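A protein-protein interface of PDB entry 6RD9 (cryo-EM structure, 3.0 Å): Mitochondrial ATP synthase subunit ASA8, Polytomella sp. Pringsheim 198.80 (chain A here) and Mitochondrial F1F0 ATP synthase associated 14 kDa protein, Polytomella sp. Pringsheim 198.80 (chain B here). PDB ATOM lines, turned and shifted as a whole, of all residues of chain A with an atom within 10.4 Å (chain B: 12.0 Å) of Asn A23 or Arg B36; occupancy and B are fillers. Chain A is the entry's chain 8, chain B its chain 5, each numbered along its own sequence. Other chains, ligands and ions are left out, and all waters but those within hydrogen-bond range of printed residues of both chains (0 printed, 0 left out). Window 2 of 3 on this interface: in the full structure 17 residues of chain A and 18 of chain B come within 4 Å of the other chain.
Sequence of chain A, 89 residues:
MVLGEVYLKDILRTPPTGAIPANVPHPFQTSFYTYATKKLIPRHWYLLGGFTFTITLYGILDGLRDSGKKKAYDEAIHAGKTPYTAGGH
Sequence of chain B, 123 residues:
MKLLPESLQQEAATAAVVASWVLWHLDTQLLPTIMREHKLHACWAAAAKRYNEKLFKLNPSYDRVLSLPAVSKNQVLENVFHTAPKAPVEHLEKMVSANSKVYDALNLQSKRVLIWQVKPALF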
ATOM      1  N   ARG A  13      16.528 -23.200   7.087  1.00  0.00           N
ATOM      2  CA  ARG A  13      16.801 -24.532   6.598  1.00  0.00           C
ATOM      3  C   ARG A  13      16.185 -25.537   7.549  1.00  0.00           C
ATOM      4  O   ARG A  13      15.907 -25.226   8.699  1.00  0.00           O
ATOM      5  CB  ARG A  13      18.278 -24.762   6.461  1.00  0.00           C
ATOM      6  CG  ARG A  13      18.974 -23.653   5.771  1.00  0.00           C
ATOM      7  CD  ARG A  13      20.278 -24.101   5.273  1.00  0.00           C
ATOM      8  NE  ARG A  13      20.961 -23.036   4.579  1.00  0.00           N
ATOM      9  CZ  ARG A  13      21.938 -22.321   5.099  1.00  0.00           C
ATOM     10  NH1 ARG A  13      22.511 -21.375   4.393  1.00  0.00           N
ATOM     11  NH2 ARG A  13      22.347 -22.564   6.315  1.00  0.00           N
ATOM     12  N   ALA A  19      24.286 -35.018   5.869  1.00  0.00           N
ATOM     13  CA  ALA A  19      25.290 -35.184   6.901  1.00  0.00           C
ATOM     14  C   ALA A  19      25.302 -33.931   7.750  1.00  0.00           C
ATOM     15  O   ALA A  19      24.871 -32.869   7.307  1.00  0.00           O
ATOM     16  CB  ALA A  19      26.672 -35.446   6.308  1.00  0.00           C
ATOM     17  N   ILE A  20      25.787 -34.073   8.971  1.00  0.00           N
ATOM     18  CA  ILE A  20      25.873 -32.938   9.887  1.00  0.00           C
ATOM     19  C   ILE A  20      26.979 -32.007   9.418  1.00  0.00           C
ATOM     20  O   ILE A  20      28.109 -32.465   9.203  1.00  0.00           O
ATOM     21  CB  ILE A  20      26.124 -33.429  11.295  1.00  0.00           C
ATOM     22  CG1 ILE A  20      24.941 -34.254  11.723  1.00  0.00           C
ATOM     23  CG2 ILE A  20      26.253 -32.296  12.232  1.00  0.00           C
ATOM     24  CD1 ILE A  20      25.080 -34.801  13.044  1.00  0.00           C
ATOM     25  N   PRO A  21      26.716 -30.725   9.233  1.00  0.00           N
ATOM     26  CA  PRO A  21      27.706 -29.839   8.632  1.00  0.00           C
ATOM     27  C   PRO A  21      28.793 -29.476   9.631  1.00  0.00           C
ATOM     28  O   PRO A  21      28.810 -29.919  10.770  1.00  0.00           O
ATOM     29  CB  PRO A  21      26.886 -28.615   8.247  1.00  0.00           C
ATOM     30  CG  PRO A  21      25.509 -28.959   8.501  1.00  0.00           C
ATOM     31  CD  PRO A  21      25.463 -30.014   9.489  1.00  0.00           C
ATOM     32  N   ALA A  22      29.719 -28.654   9.176  1.00  0.00           N
ATOM     33  CA  ALA A  22      30.687 -28.095  10.089  1.00  0.00           C
ATOM     34  C   ALA A  22      30.045 -26.976  10.886  1.00  0.00           C
ATOM     35  O   ALA A  22      29.115 -26.315  10.423  1.00  0.00           O
ATOM     36  CB  ALA A  22      31.890 -27.575   9.322  1.00  0.00           C
ATOM     37  N   ASN A  23      30.537 -26.774  12.100  1.00  0.00           N
ATOM     38  CA  ASN A  23      30.072 -25.668  12.915  1.00  0.00           C
ATOM     39  C   ASN A  23      30.527 -24.361  12.298  1.00  0.00           C
ATOM     40  O   ASN A  23      31.602 -24.281  11.705  1.00  0.00           O
ATOM     41  CB  ASN A  23      30.601 -25.814  14.328  1.00  0.00           C
ATOM     42  CG  ASN A  23      29.867 -24.972  15.309  1.00  0.00           C
ATOM     43  OD1 ASN A  23      28.957 -24.248  14.955  1.00  0.00           O
ATOM     44  ND2 ASN A  23      30.239 -25.078  16.565  1.00  0.00           N
ATOM     45  N   VAL A  24      29.679 -23.353  12.383  1.00  0.00           N
ATOM     46  CA  VAL A  24      30.020 -22.031  11.868  1.00  0.00           C
ATOM     47  C   VAL A  24      30.948 -21.349  12.866  1.00  0.00           C
ATOM     48  O   VAL A  24      30.600 -21.248  14.046  1.00  0.00           O
ATOM     49  CB  VAL A  24      28.763 -21.213  11.640  1.00  0.00           C
ATOM     50  CG1 VAL A  24      29.108 -19.816  11.321  1.00  0.00           C
ATOM     51  CG2 VAL A  24      28.012 -21.779  10.533  1.00  0.00           C
ATOM     52  N   PRO A  25      32.119 -20.894  12.452  1.00  0.00           N
ATOM     53  CA  PRO A  25      33.009 -20.220  13.383  1.00  0.00           C
ATOM     54  C   PRO A  25      32.508 -18.838  13.721  1.00  0.00           C
ATOM     55  O   PRO A  25      31.904 -18.148  12.903  1.00  0.00           O
ATOM     56  CB  PRO A  25      34.319 -20.134  12.603  1.00  0.00           C
ATOM     57  CG  PRO A  25      34.158 -21.013  11.493  1.00  0.00           C
ATOM     58  CD  PRO A  25      32.743 -21.007  11.141  1.00  0.00           C
ATOM     59  N   HIS A  26      32.762 -18.441  14.945  1.00  0.00           N
ATOM     60  CA  HIS A  26      32.649 -17.050  15.273  1.00  0.00           C
ATOM     61  C   HIS A  26      33.770 -16.291  14.571  1.00  0.00           C
ATOM     62  O   HIS A  26      34.803 -16.873  14.250  1.00  0.00           O
ATOM     63  CB  HIS A  26      32.734 -16.864  16.774  1.00  0.00           C
ATOM     64  CG  HIS A  26      32.353 -15.503  17.218  1.00  0.00           C
ATOM     65  ND1 HIS A  26      31.054 -15.120  17.397  1.00  0.00           N
ATOM     66  CD2 HIS A  26      33.097 -14.408  17.442  1.00  0.00           C
ATOM     67  CE1 HIS A  26      31.020 -13.854  17.751  1.00  0.00           C
ATOM     68  NE2 HIS A  26      32.250 -13.396  17.779  1.00  0.00           N
ATOM     69  N   PRO A  27      33.581 -15.005  14.281  1.00  0.00           N
ATOM     70  CA  PRO A  27      34.684 -14.201  13.746  1.00  0.00           C
ATOM     71  C   PRO A  27      35.914 -14.114  14.625  1.00  0.00           C
ATOM     72  O   PRO A  27      36.985 -13.806  14.112  1.00  0.00           O
ATOM     73  CB  PRO A  27      34.034 -12.838  13.577  1.00  0.00           C
ATOM     74  CG  PRO A  27      32.688 -13.168  13.213  1.00  0.00           C
ATOM     75  CD  PRO A  27      32.295 -14.385  13.947  1.00  0.00           C
ATOM     76  N   PHE A  28      35.802 -14.378  15.918  1.00  0.00           N
ATOM     77  CA  PHE A  28      36.927 -14.367  16.831  1.00  0.00           C
ATOM     78  C   PHE A  28      37.674 -15.678  16.806  1.00  0.00           C
ATOM     79  O   PHE A  28      38.875 -15.707  17.061  1.00  0.00           O
ATOM     80  CB  PHE A  28      36.449 -14.117  18.250  1.00  0.00           C
ATOM     81  CG  PHE A  28      35.920 -12.751  18.499  1.00  0.00           C
ATOM     82  CD1 PHE A  28      36.136 -11.721  17.627  1.00  0.00           C
ATOM     83  CD2 PHE A  28      35.246 -12.489  19.656  1.00  0.00           C
ATOM     84  CE1 PHE A  28      35.662 -10.492  17.888  1.00  0.00           C
ATOM     85  CE2 PHE A  28      34.786 -11.259  19.908  1.00  0.00           C
ATOM     86  CZ  PHE A  28      35.006 -10.264  19.029  1.00  0.00           C
ATOM     87  N   GLN A  29      36.984 -16.777  16.547  1.00  0.00           N
ATOM     88  CA  GLN A  29      37.664 -18.049  16.406  1.00  0.00           C
ATOM     89  C   GLN A  29      38.381 -18.143  15.086  1.00  0.00           C
ATOM     90  O   GLN A  29      39.334 -18.909  14.951  1.00  0.00           O
ATOM     91  CB  GLN A  29      36.680 -19.192  16.512  1.00  0.00           C
ATOM     92  CG  GLN A  29      35.762 -19.082  17.643  1.00  0.00           C
ATOM     93  CD  GLN A  29      34.962 -20.298  17.778  1.00  0.00           C
ATOM     94  OE1 GLN A  29      35.416 -21.365  17.441  1.00  0.00           O
ATOM     95  NE2 GLN A  29      33.771 -20.167  18.296  1.00  0.00           N
ATOM     96  N   THR A  30      37.921 -17.396  14.097  1.00  0.00           N
ATOM     97  CA  THR A  30      38.577 -17.388  12.800  1.00  0.00           C
ATOM     98  C   THR A  30      39.935 -16.717  12.880  1.00  0.00           C
ATOM     99  O   THR A  30      40.950 -17.318  12.533  1.00  0.00           O
ATOM    100  CB  THR A  30      37.688 -16.694  11.780  1.00  0.00           C
ATOM    101  OG1 THR A  30      36.567 -17.529  11.498  1.00  0.00           O
ATOM    102  CG2 THR A  30      38.430 -16.425  10.516  1.00  0.00           C
ATOM    103  N   LEU B  26      38.168 -17.597  26.952  1.00  0.00           N
ATOM    104  CA  LEU B  26      36.798 -17.312  27.314  1.00  0.00           C
ATOM    105  C   LEU B  26      36.125 -16.449  26.265  1.00  0.00           C
ATOM    106  O   LEU B  26      35.031 -16.764  25.815  1.00  0.00           O
ATOM    107  CB  LEU B  26      36.780 -16.628  28.656  1.00  0.00           C
ATOM    108  CG  LEU B  26      35.501 -16.315  29.349  1.00  0.00           C
ATOM    109  CD1 LEU B  26      35.025 -17.554  29.988  1.00  0.00           C
ATOM    110  CD2 LEU B  26      35.883 -15.310  30.339  1.00  0.00           C
ATOM    111  N   ASP B  27      36.776 -15.373  25.843  1.00  0.00           N
ATOM    112  CA  ASP B  27      36.164 -14.425  24.925  1.00  0.00           C
ATOM    113  C   ASP B  27      35.972 -14.976  23.541  1.00  0.00           C
ATOM    114  O   ASP B  27      35.089 -14.525  22.818  1.00  0.00           O
ATOM    115  CB  ASP B  27      37.028 -13.211  24.770  1.00  0.00           C
ATOM    116  CG  ASP B  27      36.668 -12.124  25.675  1.00  0.00           C
ATOM    117  OD1 ASP B  27      35.501 -12.032  26.077  1.00  0.00           O
ATOM    118  OD2 ASP B  27      37.546 -11.297  25.928  1.00  0.00           O
ATOM    119  N   THR B  28      36.822 -15.888  23.130  1.00  0.00           N
ATOM    120  CA  THR B  28      36.864 -16.365  21.766  1.00  0.00           C
ATOM    121  C   THR B  28      36.215 -17.726  21.621  1.00  0.00           C
ATOM    122  O   THR B  28      35.435 -17.941  20.707  1.00  0.00           O
ATOM    123  CB  THR B  28      38.314 -16.388  21.313  1.00  0.00           C
ATOM    124  OG1 THR B  28      38.749 -15.061  21.066  1.00  0.00           O
ATOM    125  CG2 THR B  28      38.511 -17.174  20.121  1.00  0.00           C
ATOM    126  N   GLN B  29      36.484 -18.642  22.533  1.00  0.00           N
ATOM    127  CA  GLN B  29      36.000 -20.001  22.405  1.00  0.00           C
ATOM    128  C   GLN B  29      34.823 -20.309  23.304  1.00  0.00           C
ATOM    129  O   GLN B  29      33.852 -20.900  22.846  1.00  0.00           O
ATOM    130  CB  GLN B  29      37.130 -20.980  22.680  1.00  0.00           C
ATOM    131  CG  GLN B  29      38.412 -20.605  22.008  1.00  0.00           C
ATOM    132  CD  GLN B  29      38.414 -20.947  20.566  1.00  0.00           C
ATOM    133  OE1 GLN B  29      39.129 -20.357  19.774  1.00  0.00           O
ATOM    134  NE2 GLN B  29      37.608 -21.923  20.197  1.00  0.00           N
ATOM    135  N   LEU B  30      34.878 -19.930  24.569  1.00  0.00           N
ATOM    136  CA  LEU B  30      33.788 -20.286  25.463  1.00  0.00           C
ATOM    137  C   LEU B  30      32.584 -19.384  25.281  1.00  0.00           C
ATOM    138  O   LEU B  30      31.491 -19.872  25.031  1.00  0.00           O
ATOM    139  CB  LEU B  30      34.254 -20.255  26.904  1.00  0.00           C
ATOM    140  CG  LEU B  30      35.306 -21.278  27.253  1.00  0.00           C
ATOM    141  CD1 LEU B  30      35.523 -21.229  28.709  1.00  0.00           C
ATOM    142  CD2 LEU B  30      34.880 -22.638  26.844  1.00  0.00           C
ATOM    143  N   LEU B  31      32.758 -18.070  25.384  1.00  0.00           N
ATOM    144  CA  LEU B  31      31.602 -17.180  25.379  1.00  0.00           C
ATOM    145  C   LEU B  31      30.848 -17.062  24.062  1.00  0.00           C
ATOM    146  O   LEU B  31      29.667 -16.698  24.123  1.00  0.00           O
ATOM    147  CB  LEU B  31      31.990 -15.772  25.820  1.00  0.00           C
ATOM    148  CG  LEU B  31      31.957 -15.358  27.271  1.00  0.00           C
ATOM    149  CD1 LEU B  31      32.294 -13.912  27.316  1.00  0.00           C
ATOM    150  CD2 LEU B  31      30.598 -15.605  27.805  1.00  0.00           C
ATOM    151  N   PRO B  32      31.430 -17.262  22.882  1.00  0.00           N
ATOM    152  CA  PRO B  32      30.583 -17.455  21.714  1.00  0.00           C
ATOM    153  C   PRO B  32      29.704 -18.674  21.775  1.00  0.00           C
ATOM    154  O   PRO B  32      28.564 -18.608  21.333  1.00  0.00           O
ATOM    155  CB  PRO B  32      31.611 -17.538  20.599  1.00  0.00           C
ATOM    156  CG  PRO B  32      32.535 -16.578  20.995  1.00  0.00           C
ATOM    157  CD  PRO B  32      32.723 -16.744  22.425  1.00  0.00           C
ATOM    158  N   THR B  33      30.184 -19.775  22.315  1.00  0.00           N
ATOM    159  CA  THR B  33      29.389 -20.975  22.491  1.00  0.00           C
ATOM    160  C   THR B  33      28.343 -20.828  23.583  1.00  0.00           C
ATOM    161  O   THR B  33      27.240 -21.356  23.444  1.00  0.00           O
ATOM    162  CB  THR B  33      30.332 -22.116  22.813  1.00  0.00           C
ATOM    163  OG1 THR B  33      31.297 -22.220  21.767  1.00  0.00           O
ATOM    164  CG2 THR B  33      29.616 -23.385  22.940  1.00  0.00           C
ATOM    165  N   ILE B  34      28.677 -20.131  24.672  1.00  0.00           N
ATOM    166  CA  ILE B  34      27.718 -19.856  25.738  1.00  0.00           C
ATOM    167  C   ILE B  34      26.547 -19.082  25.187  1.00  0.00           C
ATOM    168  O   ILE B  34      25.395 -19.453  25.380  1.00  0.00           O
ATOM    169  CB  ILE B  34      28.379 -19.066  26.880  1.00  0.00           C
ATOM    170  CG1 ILE B  34      29.495 -19.827  27.567  1.00  0.00           C
ATOM    171  CG2 ILE B  34      27.373 -18.622  27.881  1.00  0.00           C
ATOM    172  CD1 ILE B  34      29.136 -21.087  28.040  1.00  0.00           C
ATOM    173  N   MET B  35      26.828 -18.013  24.465  1.00  0.00           N
ATOM    174  CA  MET B  35      25.800 -17.106  24.007  1.00  0.00           C
ATOM    175  C   MET B  35      25.068 -17.617  22.793  1.00  0.00           C
ATOM    176  O   MET B  35      24.011 -17.099  22.481  1.00  0.00           O
ATOM    177  CB  MET B  35      26.400 -15.752  23.691  1.00  0.00           C
ATOM    178  CG  MET B  35      26.873 -15.009  24.874  1.00  0.00           C
ATOM    179  SD  MET B  35      25.727 -15.110  26.220  1.00  0.00           S
ATOM    180  CE  MET B  35      26.841 -14.788  27.540  1.00  0.00           C
ATOM    181  N   ARG B  36      25.583 -18.610  22.100  1.00  0.00           N
ATOM    182  CA  ARG B  36      24.833 -19.145  20.985  1.00  0.00           C
ATOM    183  C   ARG B  36      23.703 -20.007  21.470  1.00  0.00           C
ATOM    184  O   ARG B  36      22.671 -20.105  20.817  1.00  0.00           O
ATOM    185  CB  ARG B  36      25.739 -19.941  20.076  1.00  0.00           C
ATOM    186  CG  ARG B  36      26.302 -19.153  18.980  1.00  0.00           C
ATOM    187  CD  ARG B  36      27.258 -19.981  18.248  1.00  0.00           C
ATOM    188  NE  ARG B  36      28.017 -19.203  17.303  1.00  0.00           N
ATOM    189  CZ  ARG B  36      28.523 -19.715  16.201  1.00  0.00           C
ATOM    190  NH1 ARG B  36      29.196 -18.957  15.367  1.00  0.00           N
ATOM    191  NH2 ARG B  36      28.327 -20.986  15.938  1.00  0.00           N
ATOM    192  N   GLU B  37      23.874 -20.642  22.601  1.00  0.00           N
ATOM    193  CA  GLU B  37      22.809 -21.457  23.128  1.00  0.00           C
ATOM    194  C   GLU B  37      22.091 -20.811  24.284  1.00  0.00           C
ATOM    195  O   GLU B  37      20.988 -21.229  24.606  1.00  0.00           O
ATOM    196  CB  GLU B  37      23.346 -22.807  23.532  1.00  0.00           C
ATOM    197  CG  GLU B  37      24.007 -22.867  24.797  1.00  0.00           C
ATOM    198  CD  GLU B  37      24.352 -24.277  25.116  1.00  0.00           C
ATOM    199  OE1 GLU B  37      25.246 -24.818  24.451  1.00  0.00           O
ATOM    200  OE2 GLU B  37      23.711 -24.866  26.007  1.00  0.00           O
ATOM    201  N   HIS B  38      22.653 -19.779  24.885  1.00  0.00           N
ATOM    202  CA  HIS B  38      21.870 -19.002  25.822  1.00  0.00           C
ATOM    203  C   HIS B  38      20.865 -18.154  25.089  1.00  0.00           C
ATOM    204  O   HIS B  38      19.715 -18.054  25.507  1.00  0.00           O
ATOM    205  CB  HIS B  38      22.772 -18.130  26.676  1.00  0.00           C
ATOM    206  CG  HIS B  38      22.042 -17.095  27.460  1.00  0.00           C
ATOM    207  ND1 HIS B  38      21.007 -17.403  28.305  1.00  0.00           N
ATOM    208  CD2 HIS B  38      22.209 -15.760  27.542  1.00  0.00           C
ATOM    209  CE1 HIS B  38      20.552 -16.300  28.857  1.00  0.00           C
ATOM    210  NE2 HIS B  38      21.268 -15.288  28.415  1.00  0.00           N
ATOM    211  N   LYS B  39      21.268 -17.545  23.988  1.00  0.00           N
ATOM    212  CA  LYS B  39      20.412 -16.618  23.279  1.00  0.00           C
ATOM    213  C   LYS B  39      19.558 -17.256  22.209  1.00  0.00           C
ATOM    214  O   LYS B  39      18.710 -16.573  21.663  1.00  0.00           O
ATOM    215  CB  LYS B  39      21.238 -15.524  22.644  1.00  0.00           C
ATOM    216  CG  LYS B  39      21.894 -14.676  23.634  1.00  0.00           C
ATOM    217  CD  LYS B  39      22.727 -13.670  22.985  1.00  0.00           C
ATOM    218  CE  LYS B  39      23.195 -12.715  24.000  1.00  0.00           C
ATOM    219  NZ  LYS B  39      24.122 -11.828  23.346  1.00  0.00           N
ATOM    220  N   LEU B  40      19.750 -18.516  21.864  1.00  0.00           N
ATOM    221  CA  LEU B  40      18.685 -19.179  21.140  1.00  0.00           C
ATOM    222  C   LEU B  40      17.502 -19.390  22.053  1.00  0.00           C
ATOM    223  O   LEU B  40      16.361 -19.175  21.660  1.00  0.00           O
ATOM    224  CB  LEU B  40      19.158 -20.507  20.573  1.00  0.00           C
ATOM    225  CG  LEU B  40      18.110 -21.203  19.718  1.00  0.00           C
ATOM    226  CD1 LEU B  40      18.739 -21.651  18.506  1.00  0.00           C
ATOM    227  CD2 LEU B  40      17.557 -22.400  20.380  1.00  0.00           C
ATOM    228  N   HIS B  41      17.762 -19.798  23.275  1.00  0.00           N
ATOM    229  CA  HIS B  41      16.716 -19.983  24.253  1.00  0.00           C
ATOM    230  C   HIS B  41      16.108 -18.666  24.691  1.00  0.00           C
ATOM    231  O   HIS B  41      14.909 -18.599  24.936  1.00  0.00           O
ATOM    232  CB  HIS B  41      17.301 -20.723  25.433  1.00  0.00           C
ATOM    233  CG  HIS B  41      16.299 -21.152  26.441  1.00  0.00           C
ATOM    234  ND1 HIS B  41      15.836 -20.319  27.428  1.00  0.00           N
ATOM    235  CD2 HIS B  41      15.713 -22.346  26.651  1.00  0.00           C
ATOM    236  CE1 HIS B  41      14.975 -20.973  28.180  1.00  0.00           C
ATOM    237  NE2 HIS B  41      14.891 -22.207  27.734  1.00  0.00           N
ATOM    238  N   ALA B  42      16.903 -17.617  24.811  1.00  0.00           N
ATOM    239  CA  ALA B  42      16.407 -16.366  25.356  1.00  0.00           C
ATOM    240  C   ALA B  42      15.639 -15.567  24.332  1.00  0.00           C
ATOM    241  O   ALA B  42      14.688 -14.875  24.683  1.00  0.00           O
ATOM    242  CB  ALA B  42      17.558 -15.530  25.877  1.00  0.00           C
ATOM    243  N   CYS B  43      16.068 -15.596  23.076  1.00  0.00           N
ATOM    244  CA  CYS B  43      15.318 -14.927  22.032  1.00  0.00           C
ATOM    245  C   CYS B  43      14.015 -15.633  21.770  1.00  0.00           C
ATOM    246  O   CYS B  43      13.027 -14.992  21.450  1.00  0.00           O
ATOM    247  CB  CYS B  43      16.128 -14.861  20.753  1.00  0.00           C
ATOM    248  SG  CYS B  43      17.468 -13.731  20.833  1.00  0.00           S
ATOM    249  N   TRP B  44      13.988 -16.945  21.896  1.00  0.00           N
ATOM    250  CA  TRP B  44      12.753 -17.667  21.687  1.00  0.00           C
ATOM    251  C   TRP B  44      11.806 -17.491  22.850  1.00  0.00           C
ATOM    252  O   TRP B  44      10.599 -17.567  22.677  1.00  0.00           O
ATOM    253  CB  TRP B  44      13.042 -19.136  21.475  1.00  0.00           C
ATOM    254  CG  TRP B  44      13.155 -19.554  20.075  1.00  0.00           C
ATOM    255  CD1 TRP B  44      14.228 -20.102  19.491  1.00  0.00           C
ATOM    256  CD2 TRP B  44      12.144 -19.492  19.078  1.00  0.00           C
ATOM    257  NE1 TRP B  44      13.969 -20.388  18.191  1.00  0.00           N
ATOM    258  CE2 TRP B  44      12.687 -20.014  17.913  1.00  0.00           C
ATOM    259  CE3 TRP B  44      10.838 -19.015  19.051  1.00  0.00           C
ATOM    260  CZ2 TRP B  44      11.971 -20.087  16.748  1.00  0.00           C
ATOM    261  CZ3 TRP B  44      10.142 -19.111  17.929  1.00  0.00           C
ATOM    262  CH2 TRP B  44      10.698 -19.633  16.778  1.00  0.00           C
ATOM    263  N   ALA B  45      12.319 -17.301  24.044  1.00  0.00           N
ATOM    264  CA  ALA B  45      11.447 -17.111  25.184  1.00  0.00           C
ATOM    265  C   ALA B  45      10.974 -15.688  25.314  1.00  0.00           C
ATOM    266  O   ALA B  45       9.958 -15.452  25.956  1.00  0.00           O
ATOM    267  CB  ALA B  45      12.152 -17.515  26.462  1.00  0.00           C
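The side-chain amide oxygen of Asn A23 sits at hydrogen-bond distance from the guanidinium group of Arg B36, 3.5 Å away.
The guanidinium group (NH2) of Arg B36 lies within hydrogen-bond range of the backbone carbonyl oxygen (O) of Val A24.
The backbone carbonyl oxygen of Gln B29 lies within hydrogen-bond range of the side-chain hydroxyl of Thr B33, at 3.1 Å.
The backbone carbonyl oxygen of His A26 lies within hydrogen-bond range of the side-chain hydroxyl of Thr A30 (3.3 Å).
Among the printed residues, pairs that only touch across the chains: Pro A25 with Arg B36 (3.7 Å), His A26 with Pro B32 (3.9 Å), His A26 with Arg B36 (3.6 Å), Phe A28 with Asp B27 (3.8 Å), Phe A28 with Thr B28 (3.4 Å), Gln A29 with Thr B28 (3.3 Å) and Gln A29 with Gln B29 (3.6 Å).
No residue of chain B comes within 4 Å of Pro A21.
Of chain B, only Arg B36 (3.0 Å) comes within 4 Å of Val A24.
Of the printed residues of chain B, Pro A25 touches Arg B36.
Printed residues of chain A within 4 Å of Thr B28: Phe A28 (3.4 Å) and Gln A29 (3.3 Å).
Printed residues of chain A within 4 Å of Gln B29: Gln A29.
Printed residues of chain A within 4 Å of Pro B32: His A26 (3.9 Å).
No residue of chain A comes within 4 Å of Thr B33.
Arg B36 touches just these residues of chain A: Asn A23 (3.5 Å), Val A24 (3.0 Å), Pro A25 (3.7 Å) and His A26 (3.6 Å).
Cys B43 touches none of the printed residues of chain A.
The nearest residue of chain A that does not touch Arg B36 is Gln A29 (5.6 Å).
The nearest printed residue of chain A that does not touch Pro B32 is Gln A29 (4.1 Å).
Hydrophobic or aromatic side chains of chain A within 4 Å of the printed part of chain B: His A26 and Phe A28.
Of the 20 printed residues of chain B, 5 touch a printed residue of chain A.
Hydrophobic or aromatic side chains of chain B within 4 Å of the printed part of chain A: Pro B32.
Among the printed residues, no Asp or Glu carboxylate lies within 4 Å of a Lys or Arg side-chain nitrogen of the other chain.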
